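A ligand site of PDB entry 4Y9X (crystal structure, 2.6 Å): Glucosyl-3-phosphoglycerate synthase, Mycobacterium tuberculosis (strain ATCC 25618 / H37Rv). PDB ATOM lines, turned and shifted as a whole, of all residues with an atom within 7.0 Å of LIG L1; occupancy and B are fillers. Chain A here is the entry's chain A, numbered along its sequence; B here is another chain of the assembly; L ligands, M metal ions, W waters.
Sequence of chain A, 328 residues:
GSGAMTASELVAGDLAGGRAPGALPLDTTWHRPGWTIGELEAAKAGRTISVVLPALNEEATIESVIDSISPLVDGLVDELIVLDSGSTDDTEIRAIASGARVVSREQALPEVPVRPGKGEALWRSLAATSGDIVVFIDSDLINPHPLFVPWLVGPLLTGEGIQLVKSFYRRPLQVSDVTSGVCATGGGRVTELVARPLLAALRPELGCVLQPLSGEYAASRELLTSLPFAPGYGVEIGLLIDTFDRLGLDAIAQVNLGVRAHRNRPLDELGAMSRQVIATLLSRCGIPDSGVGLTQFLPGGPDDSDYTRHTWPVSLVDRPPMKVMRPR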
ATOM      1  N   GLY A 187       9.628 -23.791  11.510  1.00  0.00           N
ATOM      2  CA  GLY A 187       9.722 -24.706  12.630  1.00  0.00           C
ATOM      3  C   GLY A 187      10.888 -25.678  12.484  1.00  0.00           C
ATOM      4  O   GLY A 187      10.790 -26.831  12.888  1.00  0.00           O
ATOM      5  N   GLY A 188      11.977 -25.179  11.902  1.00  0.00           N
ATOM      6  CA  GLY A 188      13.113 -26.012  11.535  1.00  0.00           C
ATOM      7  C   GLY A 188      12.771 -26.852  10.319  1.00  0.00           C
ATOM      8  O   GLY A 188      12.845 -28.074  10.343  1.00  0.00           O
ATOM      9  N   ARG A 189      12.401 -26.176   9.238  1.00  0.00           N
ATOM     10  CA  ARG A 189      12.073 -26.834   7.984  1.00  0.00           C
ATOM     11  C   ARG A 189      13.195 -27.671   7.362  1.00  0.00           C
ATOM     12  O   ARG A 189      12.976 -28.811   6.966  1.00  0.00           O
ATOM     13  CB  ARG A 189      11.611 -25.776   6.972  1.00  0.00           C
ATOM     14  CG  ARG A 189      10.178 -25.334   7.197  1.00  0.00           C
ATOM     15  CD  ARG A 189       9.845 -24.113   6.373  1.00  0.00           C
ATOM     16  NE  ARG A 189      10.630 -22.945   6.774  1.00  0.00           N
ATOM     17  CZ  ARG A 189      10.578 -21.766   6.192  1.00  0.00           C
ATOM     18  NH1 ARG A 189       9.766 -21.567   5.148  1.00  0.00           N
ATOM     19  NH2 ARG A 189      11.329 -20.769   6.628  1.00  0.00           N
ATOM     20  N   VAL A 190      14.406 -27.108   7.295  1.00  0.00           N
ATOM     21  CA  VAL A 190      15.522 -27.836   6.709  1.00  0.00           C
ATOM     22  C   VAL A 190      15.868 -29.008   7.622  1.00  0.00           C
ATOM     23  O   VAL A 190      16.155 -30.107   7.156  1.00  0.00           O
ATOM     24  CB  VAL A 190      16.752 -26.933   6.490  1.00  0.00           C
ATOM     25  CG1 VAL A 190      18.002 -27.740   6.148  1.00  0.00           C
ATOM     26  CG2 VAL A 190      16.473 -25.916   5.397  1.00  0.00           C
ATOM     27  N   THR A 191      15.832 -28.744   8.922  1.00  0.00           N
ATOM     28  CA  THR A 191      16.184 -29.744   9.921  1.00  0.00           C
ATOM     29  C   THR A 191      15.238 -30.945   9.859  1.00  0.00           C
ATOM     30  O   THR A 191      15.687 -32.095   9.822  1.00  0.00           O
ATOM     31  CB  THR A 191      16.177 -29.146  11.343  1.00  0.00           C
ATOM     32  OG1 THR A 191      17.107 -28.062  11.413  1.00  0.00           O
ATOM     33  CG2 THR A 191      16.560 -30.215  12.377  1.00  0.00           C
ATOM     34  N   GLU A 192      13.942 -30.669   9.846  1.00  0.00           N
ATOM     35  CA  GLU A 192      12.937 -31.731   9.987  1.00  0.00           C
ATOM     36  C   GLU A 192      12.624 -32.422   8.669  1.00  0.00           C
ATOM     37  O   GLU A 192      12.192 -33.582   8.671  1.00  0.00           O
ATOM     38  CB  GLU A 192      11.645 -31.152  10.578  1.00  0.00           C
ATOM     39  CG  GLU A 192      11.779 -30.519  11.952  1.00  0.00           C
ATOM     40  CD  GLU A 192      12.081 -31.532  13.053  1.00  0.00           C
ATOM     41  OE1 GLU A 192      11.867 -32.745  12.826  1.00  0.00           O
ATOM     42  OE2 GLU A 192      12.542 -31.108  14.129  1.00  0.00           O
ATOM     43  N   GLN A 211      18.354 -31.336  17.280  1.00  0.00           N
ATOM     44  CA  GLN A 211      18.630 -30.167  16.441  1.00  0.00           C
ATOM     45  C   GLN A 211      20.059 -30.232  15.906  1.00  0.00           C
ATOM     46  O   GLN A 211      20.909 -29.447  16.322  1.00  0.00           O
ATOM     47  CB  GLN A 211      18.401 -28.873  17.213  1.00  0.00           C
ATOM     48  CG  GLN A 211      16.955 -28.653  17.664  1.00  0.00           C
ATOM     49  CD  GLN A 211      16.018 -28.332  16.510  1.00  0.00           C
ATOM     50  OE1 GLN A 211      16.337 -27.511  15.653  1.00  0.00           O
ATOM     51  NE2 GLN A 211      14.855 -28.973  16.491  1.00  0.00           N
ATOM     52  N   LEU A 213      21.394 -29.286  13.189  1.00  0.00           N
ATOM     53  CA  LEU A 213      21.813 -28.075  12.475  1.00  0.00           C
ATOM     54  C   LEU A 213      21.874 -26.817  13.342  1.00  0.00           C
ATOM     55  O   LEU A 213      22.081 -25.718  12.825  1.00  0.00           O
ATOM     56  CB  LEU A 213      20.889 -27.826  11.282  1.00  0.00           C
ATOM     57  CG  LEU A 213      20.672 -28.993  10.312  1.00  0.00           C
ATOM     58  CD1 LEU A 213      19.863 -28.513   9.121  1.00  0.00           C
ATOM     59  CD2 LEU A 213      21.993 -29.607   9.850  1.00  0.00           C
ATOM     60  N   SER A 214      21.654 -26.949  14.648  1.00  0.00           N
ATOM     61  CA  SER A 214      21.603 -25.782  15.520  1.00  0.00           C
ATOM     62  C   SER A 214      22.898 -24.980  15.474  1.00  0.00           C
ATOM     63  O   SER A 214      23.987 -25.531  15.601  1.00  0.00           O
ATOM     64  CB  SER A 214      21.294 -26.202  16.961  1.00  0.00           C
ATOM     65  OG  SER A 214      22.170 -27.228  17.391  1.00  0.00           O
ATOM     66  N   GLY A 215      22.766 -23.663  15.274  1.00  0.00           N
ATOM     67  CA  GLY A 215      23.913 -22.774  15.271  1.00  0.00           C
ATOM     68  C   GLY A 215      24.506 -22.473  16.628  1.00  0.00           C
ATOM     69  O   GLY A 215      25.558 -21.826  16.699  1.00  0.00           O
ATOM     70  N   ARG A 260      13.692 -20.669  20.643  1.00  0.00           N
ATOM     71  CA  ARG A 260      14.488 -19.731  19.853  1.00  0.00           C
ATOM     72  C   ARG A 260      13.718 -19.177  18.677  1.00  0.00           C
ATOM     73  O   ARG A 260      12.918 -19.860  18.032  1.00  0.00           O
ATOM     74  CB  ARG A 260      15.786 -20.354  19.359  1.00  0.00           C
ATOM     75  CG  ARG A 260      15.639 -21.476  18.326  1.00  0.00           C
ATOM     76  CD  ARG A 260      16.138 -21.083  16.934  1.00  0.00           C
ATOM     77  NE  ARG A 260      17.603 -21.055  16.852  1.00  0.00           N
ATOM     78  CZ  ARG A 260      18.300 -21.181  15.722  1.00  0.00           C
ATOM     79  NH1 ARG A 260      19.627 -21.153  15.751  1.00  0.00           N
ATOM     80  NH2 ARG A 260      17.675 -21.329  14.558  1.00  0.00           N
ATOM     81  N   HIS A 262      14.436 -16.520  15.196  1.00  0.00           N
ATOM     82  CA  HIS A 262      15.466 -15.934  14.341  1.00  0.00           C
ATOM     83  C   HIS A 262      14.851 -15.495  13.024  1.00  0.00           C
ATOM     84  O   HIS A 262      13.649 -15.631  12.798  1.00  0.00           O
ATOM     85  CB  HIS A 262      16.621 -16.925  14.107  1.00  0.00           C
ATOM     86  CG  HIS A 262      16.263 -18.115  13.269  1.00  0.00           C
ATOM     87  ND1 HIS A 262      17.006 -18.506  12.171  1.00  0.00           N
ATOM     88  CD2 HIS A 262      15.251 -19.013  13.368  1.00  0.00           C
ATOM     89  CE1 HIS A 262      16.464 -19.581  11.632  1.00  0.00           C
ATOM     90  NE2 HIS A 262      15.394 -19.912  12.341  1.00  0.00           N
ATOM     91  N   ARG A 263      15.692 -14.929  12.171  1.00  0.00           N
ATOM     92  CA  ARG A 263      15.318 -14.575  10.808  1.00  0.00           C
ATOM     93  C   ARG A 263      14.676 -15.754  10.106  1.00  0.00           C
ATOM     94  O   ARG A 263      15.284 -16.829  10.034  1.00  0.00           O
ATOM     95  CB  ARG A 263      16.569 -14.142  10.041  1.00  0.00           C
ATOM     96  CG  ARG A 263      16.305 -13.399   8.739  1.00  0.00           C
ATOM     97  CD  ARG A 263      17.439 -13.576   7.729  1.00  0.00           C
ATOM     98  NE  ARG A 263      18.771 -13.532   8.343  1.00  0.00           N
ATOM     99  CZ  ARG A 263      19.510 -14.589   8.665  1.00  0.00           C
ATOM    100  NH1 ARG A 263      19.071 -15.826   8.441  1.00  0.00           N
ATOM    101  NH2 ARG A 263      20.695 -14.421   9.222  1.00  0.00           N
ATOM    102  N   ASN A 264      13.460 -15.579   9.572  1.00  0.00           N
ATOM    103  CA  ASN A 264      12.928 -16.570   8.636  1.00  0.00           C
ATOM    104  C   ASN A 264      13.204 -16.211   7.199  1.00  0.00           C
ATOM    105  O   ASN A 264      12.606 -15.309   6.619  1.00  0.00           O
ATOM    106  CB  ASN A 264      11.417 -16.695   8.830  1.00  0.00           C
ATOM    107  CG  ASN A 264      11.042 -17.107  10.239  1.00  0.00           C
ATOM    108  OD1 ASN A 264      11.752 -17.854  10.909  1.00  0.00           O
ATOM    109  ND2 ASN A 264       9.896 -16.603  10.709  1.00  0.00           N
ATOM    110  N   ARG A 265      14.142 -16.955   6.632  1.00  0.00           N
ATOM    111  CA  ARG A 265      14.575 -16.813   5.259  1.00  0.00           C
ATOM    112  C   ARG A 265      13.522 -17.282   4.241  1.00  0.00           C
ATOM    113  O   ARG A 265      12.700 -18.141   4.559  1.00  0.00           O
ATOM    114  CB  ARG A 265      15.891 -17.563   5.080  1.00  0.00           C
ATOM    115  CG  ARG A 265      16.940 -17.058   6.066  1.00  0.00           C
ATOM    116  CD  ARG A 265      18.227 -17.809   5.933  1.00  0.00           C
ATOM    117  NE  ARG A 265      18.913 -17.467   4.688  1.00  0.00           N
ATOM    118  CZ  ARG A 265      19.791 -18.249   4.073  1.00  0.00           C
ATOM    119  NH1 ARG A 265      20.093 -19.438   4.581  1.00  0.00           N
ATOM    120  NH2 ARG A 265      20.362 -17.858   2.945  1.00  0.00           N
ATOM    121  N   LEU A 270      16.535 -21.314   1.417  1.00  0.00           N
ATOM    122  CA  LEU A 270      16.565 -22.596   2.108  1.00  0.00           C
ATOM    123  C   LEU A 270      16.930 -23.725   1.152  1.00  0.00           C
ATOM    124  O   LEU A 270      17.496 -24.733   1.558  1.00  0.00           O
ATOM    125  CB  LEU A 270      15.232 -22.876   2.787  1.00  0.00           C
ATOM    126  CG  LEU A 270      14.816 -21.908   3.901  1.00  0.00           C
ATOM    127  CD1 LEU A 270      13.554 -22.404   4.581  1.00  0.00           C
ATOM    128  CD2 LEU A 270      15.939 -21.699   4.921  1.00  0.00           C
ATOM    129  N   MET A 273      20.562 -23.875   0.926  1.00  0.00           N
ATOM    130  CA  MET A 273      21.146 -24.307   2.188  1.00  0.00           C
ATOM    131  C   MET A 273      21.061 -25.829   2.286  1.00  0.00           C
ATOM    132  O   MET A 273      22.043 -26.500   2.625  1.00  0.00           O
ATOM    133  CB  MET A 273      20.408 -23.688   3.368  1.00  0.00           C
ATOM    134  CG  MET A 273      21.098 -23.853   4.703  1.00  0.00           C
ATOM    135  SD  MET A 273      19.954 -23.866   6.092  1.00  0.00           S
ATOM    136  CE  MET A 273      19.210 -22.263   5.880  1.00  0.00           C
ATOM    137  N   LEU B 193      13.017 -28.487  -0.795  1.00  0.00           N
ATOM    138  CA  LEU B 193      14.056 -28.689   0.214  1.00  0.00           C
ATOM    139  C   LEU B 193      14.647 -30.092   0.148  1.00  0.00           C
ATOM    140  O   LEU B 193      15.817 -30.297   0.496  1.00  0.00           O
ATOM    141  CB  LEU B 193      13.494 -28.440   1.616  1.00  0.00           C
ATOM    142  CG  LEU B 193      12.958 -27.036   1.932  1.00  0.00           C
ATOM    143  CD1 LEU B 193      12.700 -26.908   3.429  1.00  0.00           C
ATOM    144  CD2 LEU B 193      13.891 -25.944   1.453  1.00  0.00           C
ATOM    145  N   LEU B 267       3.904 -30.006   9.711  1.00  0.00           N
ATOM    146  CA  LEU B 267       5.322 -30.259   9.429  1.00  0.00           C
ATOM    147  C   LEU B 267       5.713 -31.705   9.746  1.00  0.00           C
ATOM    148  O   LEU B 267       6.575 -32.287   9.085  1.00  0.00           O
ATOM    149  CB  LEU B 267       6.203 -29.289  10.223  1.00  0.00           C
ATOM    150  CG  LEU B 267       7.630 -29.066   9.708  1.00  0.00           C
ATOM    151  CD1 LEU B 267       7.639 -28.378   8.353  1.00  0.00           C
ATOM    152  CD2 LEU B 267       8.426 -28.255  10.722  1.00  0.00           C
HETATM  153  C1  LIG L   1      16.756 -24.689  10.015  1.00  0.00           C
HETATM  154  O1  LIG L   1      17.446 -24.504  11.047  1.00  0.00           O
HETATM  155  O2  LIG L   1      16.430 -25.851   9.676  1.00  0.00           O
HETATM  156  C2  LIG L   1      16.318 -23.514   9.166  1.00  0.00           C
HETATM  157  O3  LIG L   1      16.729 -22.301   9.771  1.00  0.00           O
HETATM  158  C3  LIG L   1      14.808 -23.524   9.048  1.00  0.00           C
HETATM  159  O4  LIG L   1      14.300 -22.271   9.425  1.00  0.00           O
HETATM  160  P1  LIG L   1      12.825 -22.209  10.005  1.00  0.00           P
HETATM  161  O5  LIG L   1      12.388 -20.774  10.141  1.00  0.00           O
HETATM  162  O6  LIG L   1      11.889 -22.953   9.071  1.00  0.00           O
HETATM  163  O7  LIG L   1      12.802 -22.869  11.362  1.00  0.00           O
HETATM  164  N1  LG2 L   2      26.465 -16.463   8.662  1.00  0.00           N
HETATM  165  C1  LG2 L   2      27.765 -16.004   8.334  1.00  0.00           C
HETATM  166  N2  LG2 L   2      28.200 -16.080   7.061  1.00  0.00           N
HETATM  167  C2  LG2 L   2      27.435 -16.582   6.086  1.00  0.00           C
HETATM  168  C3  LG2 L   2      26.152 -17.043   6.391  1.00  0.00           C
HETATM  169  C4  LG2 L   2      25.690 -16.977   7.699  1.00  0.00           C
HETATM  170  O1  LG2 L   2      28.520 -15.532   9.210  1.00  0.00           O
HETATM  171  O2  LG2 L   2      27.856 -16.637   4.917  1.00  0.00           O
HETATM  172  C5  LG2 L   2      25.980 -16.390  10.048  1.00  0.00           C
HETATM  173  C6  LG2 L   2      24.775 -15.482  10.190  1.00  0.00           C
HETATM  174  O3  LG2 L   2      25.184 -14.168  10.552  1.00  0.00           O
HETATM  175  C7  LG2 L   2      23.946 -16.127  11.285  1.00  0.00           C
HETATM  176  C8  LG2 L   2      24.444 -17.559  11.371  1.00  0.00           C
HETATM  177  O4  LG2 L   2      25.567 -17.680  10.490  1.00  0.00           O
HETATM  178  O5  LG2 L   2      24.138 -15.450  12.530  1.00  0.00           O
HETATM  179  C9  LG2 L   2      23.371 -18.540  10.932  1.00  0.00           C
HETATM  180  O6  LG2 L   2      23.088 -18.334   9.546  1.00  0.00           O
HETATM  181  P1  LG2 L   2      21.574 -18.246   8.998  1.00  0.00           P
HETATM  182  O7  LG2 L   2      20.665 -17.614  10.019  1.00  0.00           O
HETATM  183  O8  LG2 L   2      21.546 -17.484   7.698  1.00  0.00           O
HETATM  184  O9  LG2 L   2      21.227 -19.798   8.749  1.00  0.00           O
HETATM  185  P2  LG2 L   2      19.878 -20.484   9.267  1.00  0.00           P
HETATM  186  O10 LG2 L   2      18.768 -20.318   8.257  1.00  0.00           O
HETATM  187  O11 LG2 L   2      19.459 -19.945  10.622  1.00  0.00           O
HETATM  188  O12 LG2 L   2      20.408 -21.999   9.354  1.00  0.00           O
HETATM  189  C10 LG2 L   2      20.305 -22.861  10.486  1.00  0.00           C
HETATM  190  C11 LG2 L   2      21.194 -22.410  11.639  1.00  0.00           C
HETATM  191  C12 LG2 L   2      22.619 -22.222  11.135  1.00  0.00           C
HETATM  192  C13 LG2 L   2      23.114 -23.493  10.469  1.00  0.00           C
HETATM  193  C14 LG2 L   2      22.091 -24.033   9.450  1.00  0.00           C
HETATM  194  C15 LG2 L   2      22.507 -25.372   8.847  1.00  0.00           C
HETATM  195  O13 LG2 L   2      20.686 -21.188  12.215  1.00  0.00           O
HETATM  196  O14 LG2 L   2      23.477 -21.922  12.241  1.00  0.00           O
HETATM  197  O15 LG2 L   2      24.355 -23.226   9.784  1.00  0.00           O
HETATM  198  O16 LG2 L   2      20.785 -24.130  10.045  1.00  0.00           O
HETATM  199  O17 LG2 L   2      23.401 -26.079   9.715  1.00  0.00           O
HETATM  200 MN    MN M   1      19.069 -18.002  11.523  1.00  0.00          MN
HETATM  201  O   HOH W   1      15.724 -23.021  13.007  1.00  0.00           O
HETATM  202  O   HOH W   2      15.177 -19.446   8.648  1.00  0.00           O
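An oxygen (O10) of LG2 L2 lies within hydrogen-bond range of an oxygen (O3) of LIG L1, at 3.2 Å.
Water W1 lies within hydrogen-bond range of O1 of LIG L1, NH2 of Arg 260 and NE2 of His 262. Water W2 lies within hydrogen-bond range of O of Arg 263 (3.0 Å), O4 of LIG L1 (3.1 Å) and N of Arg 265 (3.4 Å).
CE1 of His 262 touches O3 of LIG L1, 3.3 Å away. Seven residues have an atom within 4 Å of LIG L1: Gly 187, Gly 188, Arg 189, Val 190, Thr 191, His 262 and Asn 264. Along chain A the residues within 4 Å of LIG L1 span positions 187 to 264. The nearest printed residue that does not touch LIG L1 is Leu 213 (4.4 Å).
OD1 of Asn 264 lies close to O of His 262 (3.5 Å). The guanidinium group (NH2) of Arg 260 lies within hydrogen-bond range of a ring nitrogen (NE2) of His 262 (3.5 Å).
N of Gly 188 sits at hydrogen-bond distance from O7 of LIG L1 (2.5 Å). N of Arg 189 sits at hydrogen-bond distance from O6 of LIG L1, 3.3 Å away. The guanidinium group (NE) of Arg 189 is in salt-bridge range of an oxygen (O6) of LIG L1. The backbone NH (N) of Thr 191 is in hydrogen-bond range of an oxygen (O2) of LIG L1, at 3.0 Å. An oxygen (O2) of LIG L1 sits at hydrogen-bond distance from the side-chain hydroxyl (OG1) of Thr 191, at 2.9 Å. The side-chain amide oxygen of Asn 264 lies close to an oxygen (O5) of LIG L1 (3.1 Å). The backbone NH (N) of Gly 187 lies within hydrogen-bond range of an oxygen (O7) of LIG L1 (3.3 Å). The backbone NH (N) of Val 190 is in hydrogen-bond range of an oxygen (O2) of LIG L1. The backbone carbonyl oxygen (O) of Leu 213 lies within hydrogen-bond range of an oxygen (O17) of LG2 L2, at 3.4 Å. NH1 of Arg 263 is in salt-bridge range of O8 of LG2 L2, at 3.1 Å. The guanidinium group of Arg 265 lies within salt-bridge range of an oxygen (O8) of LG2 L2, 3.96 Å away.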
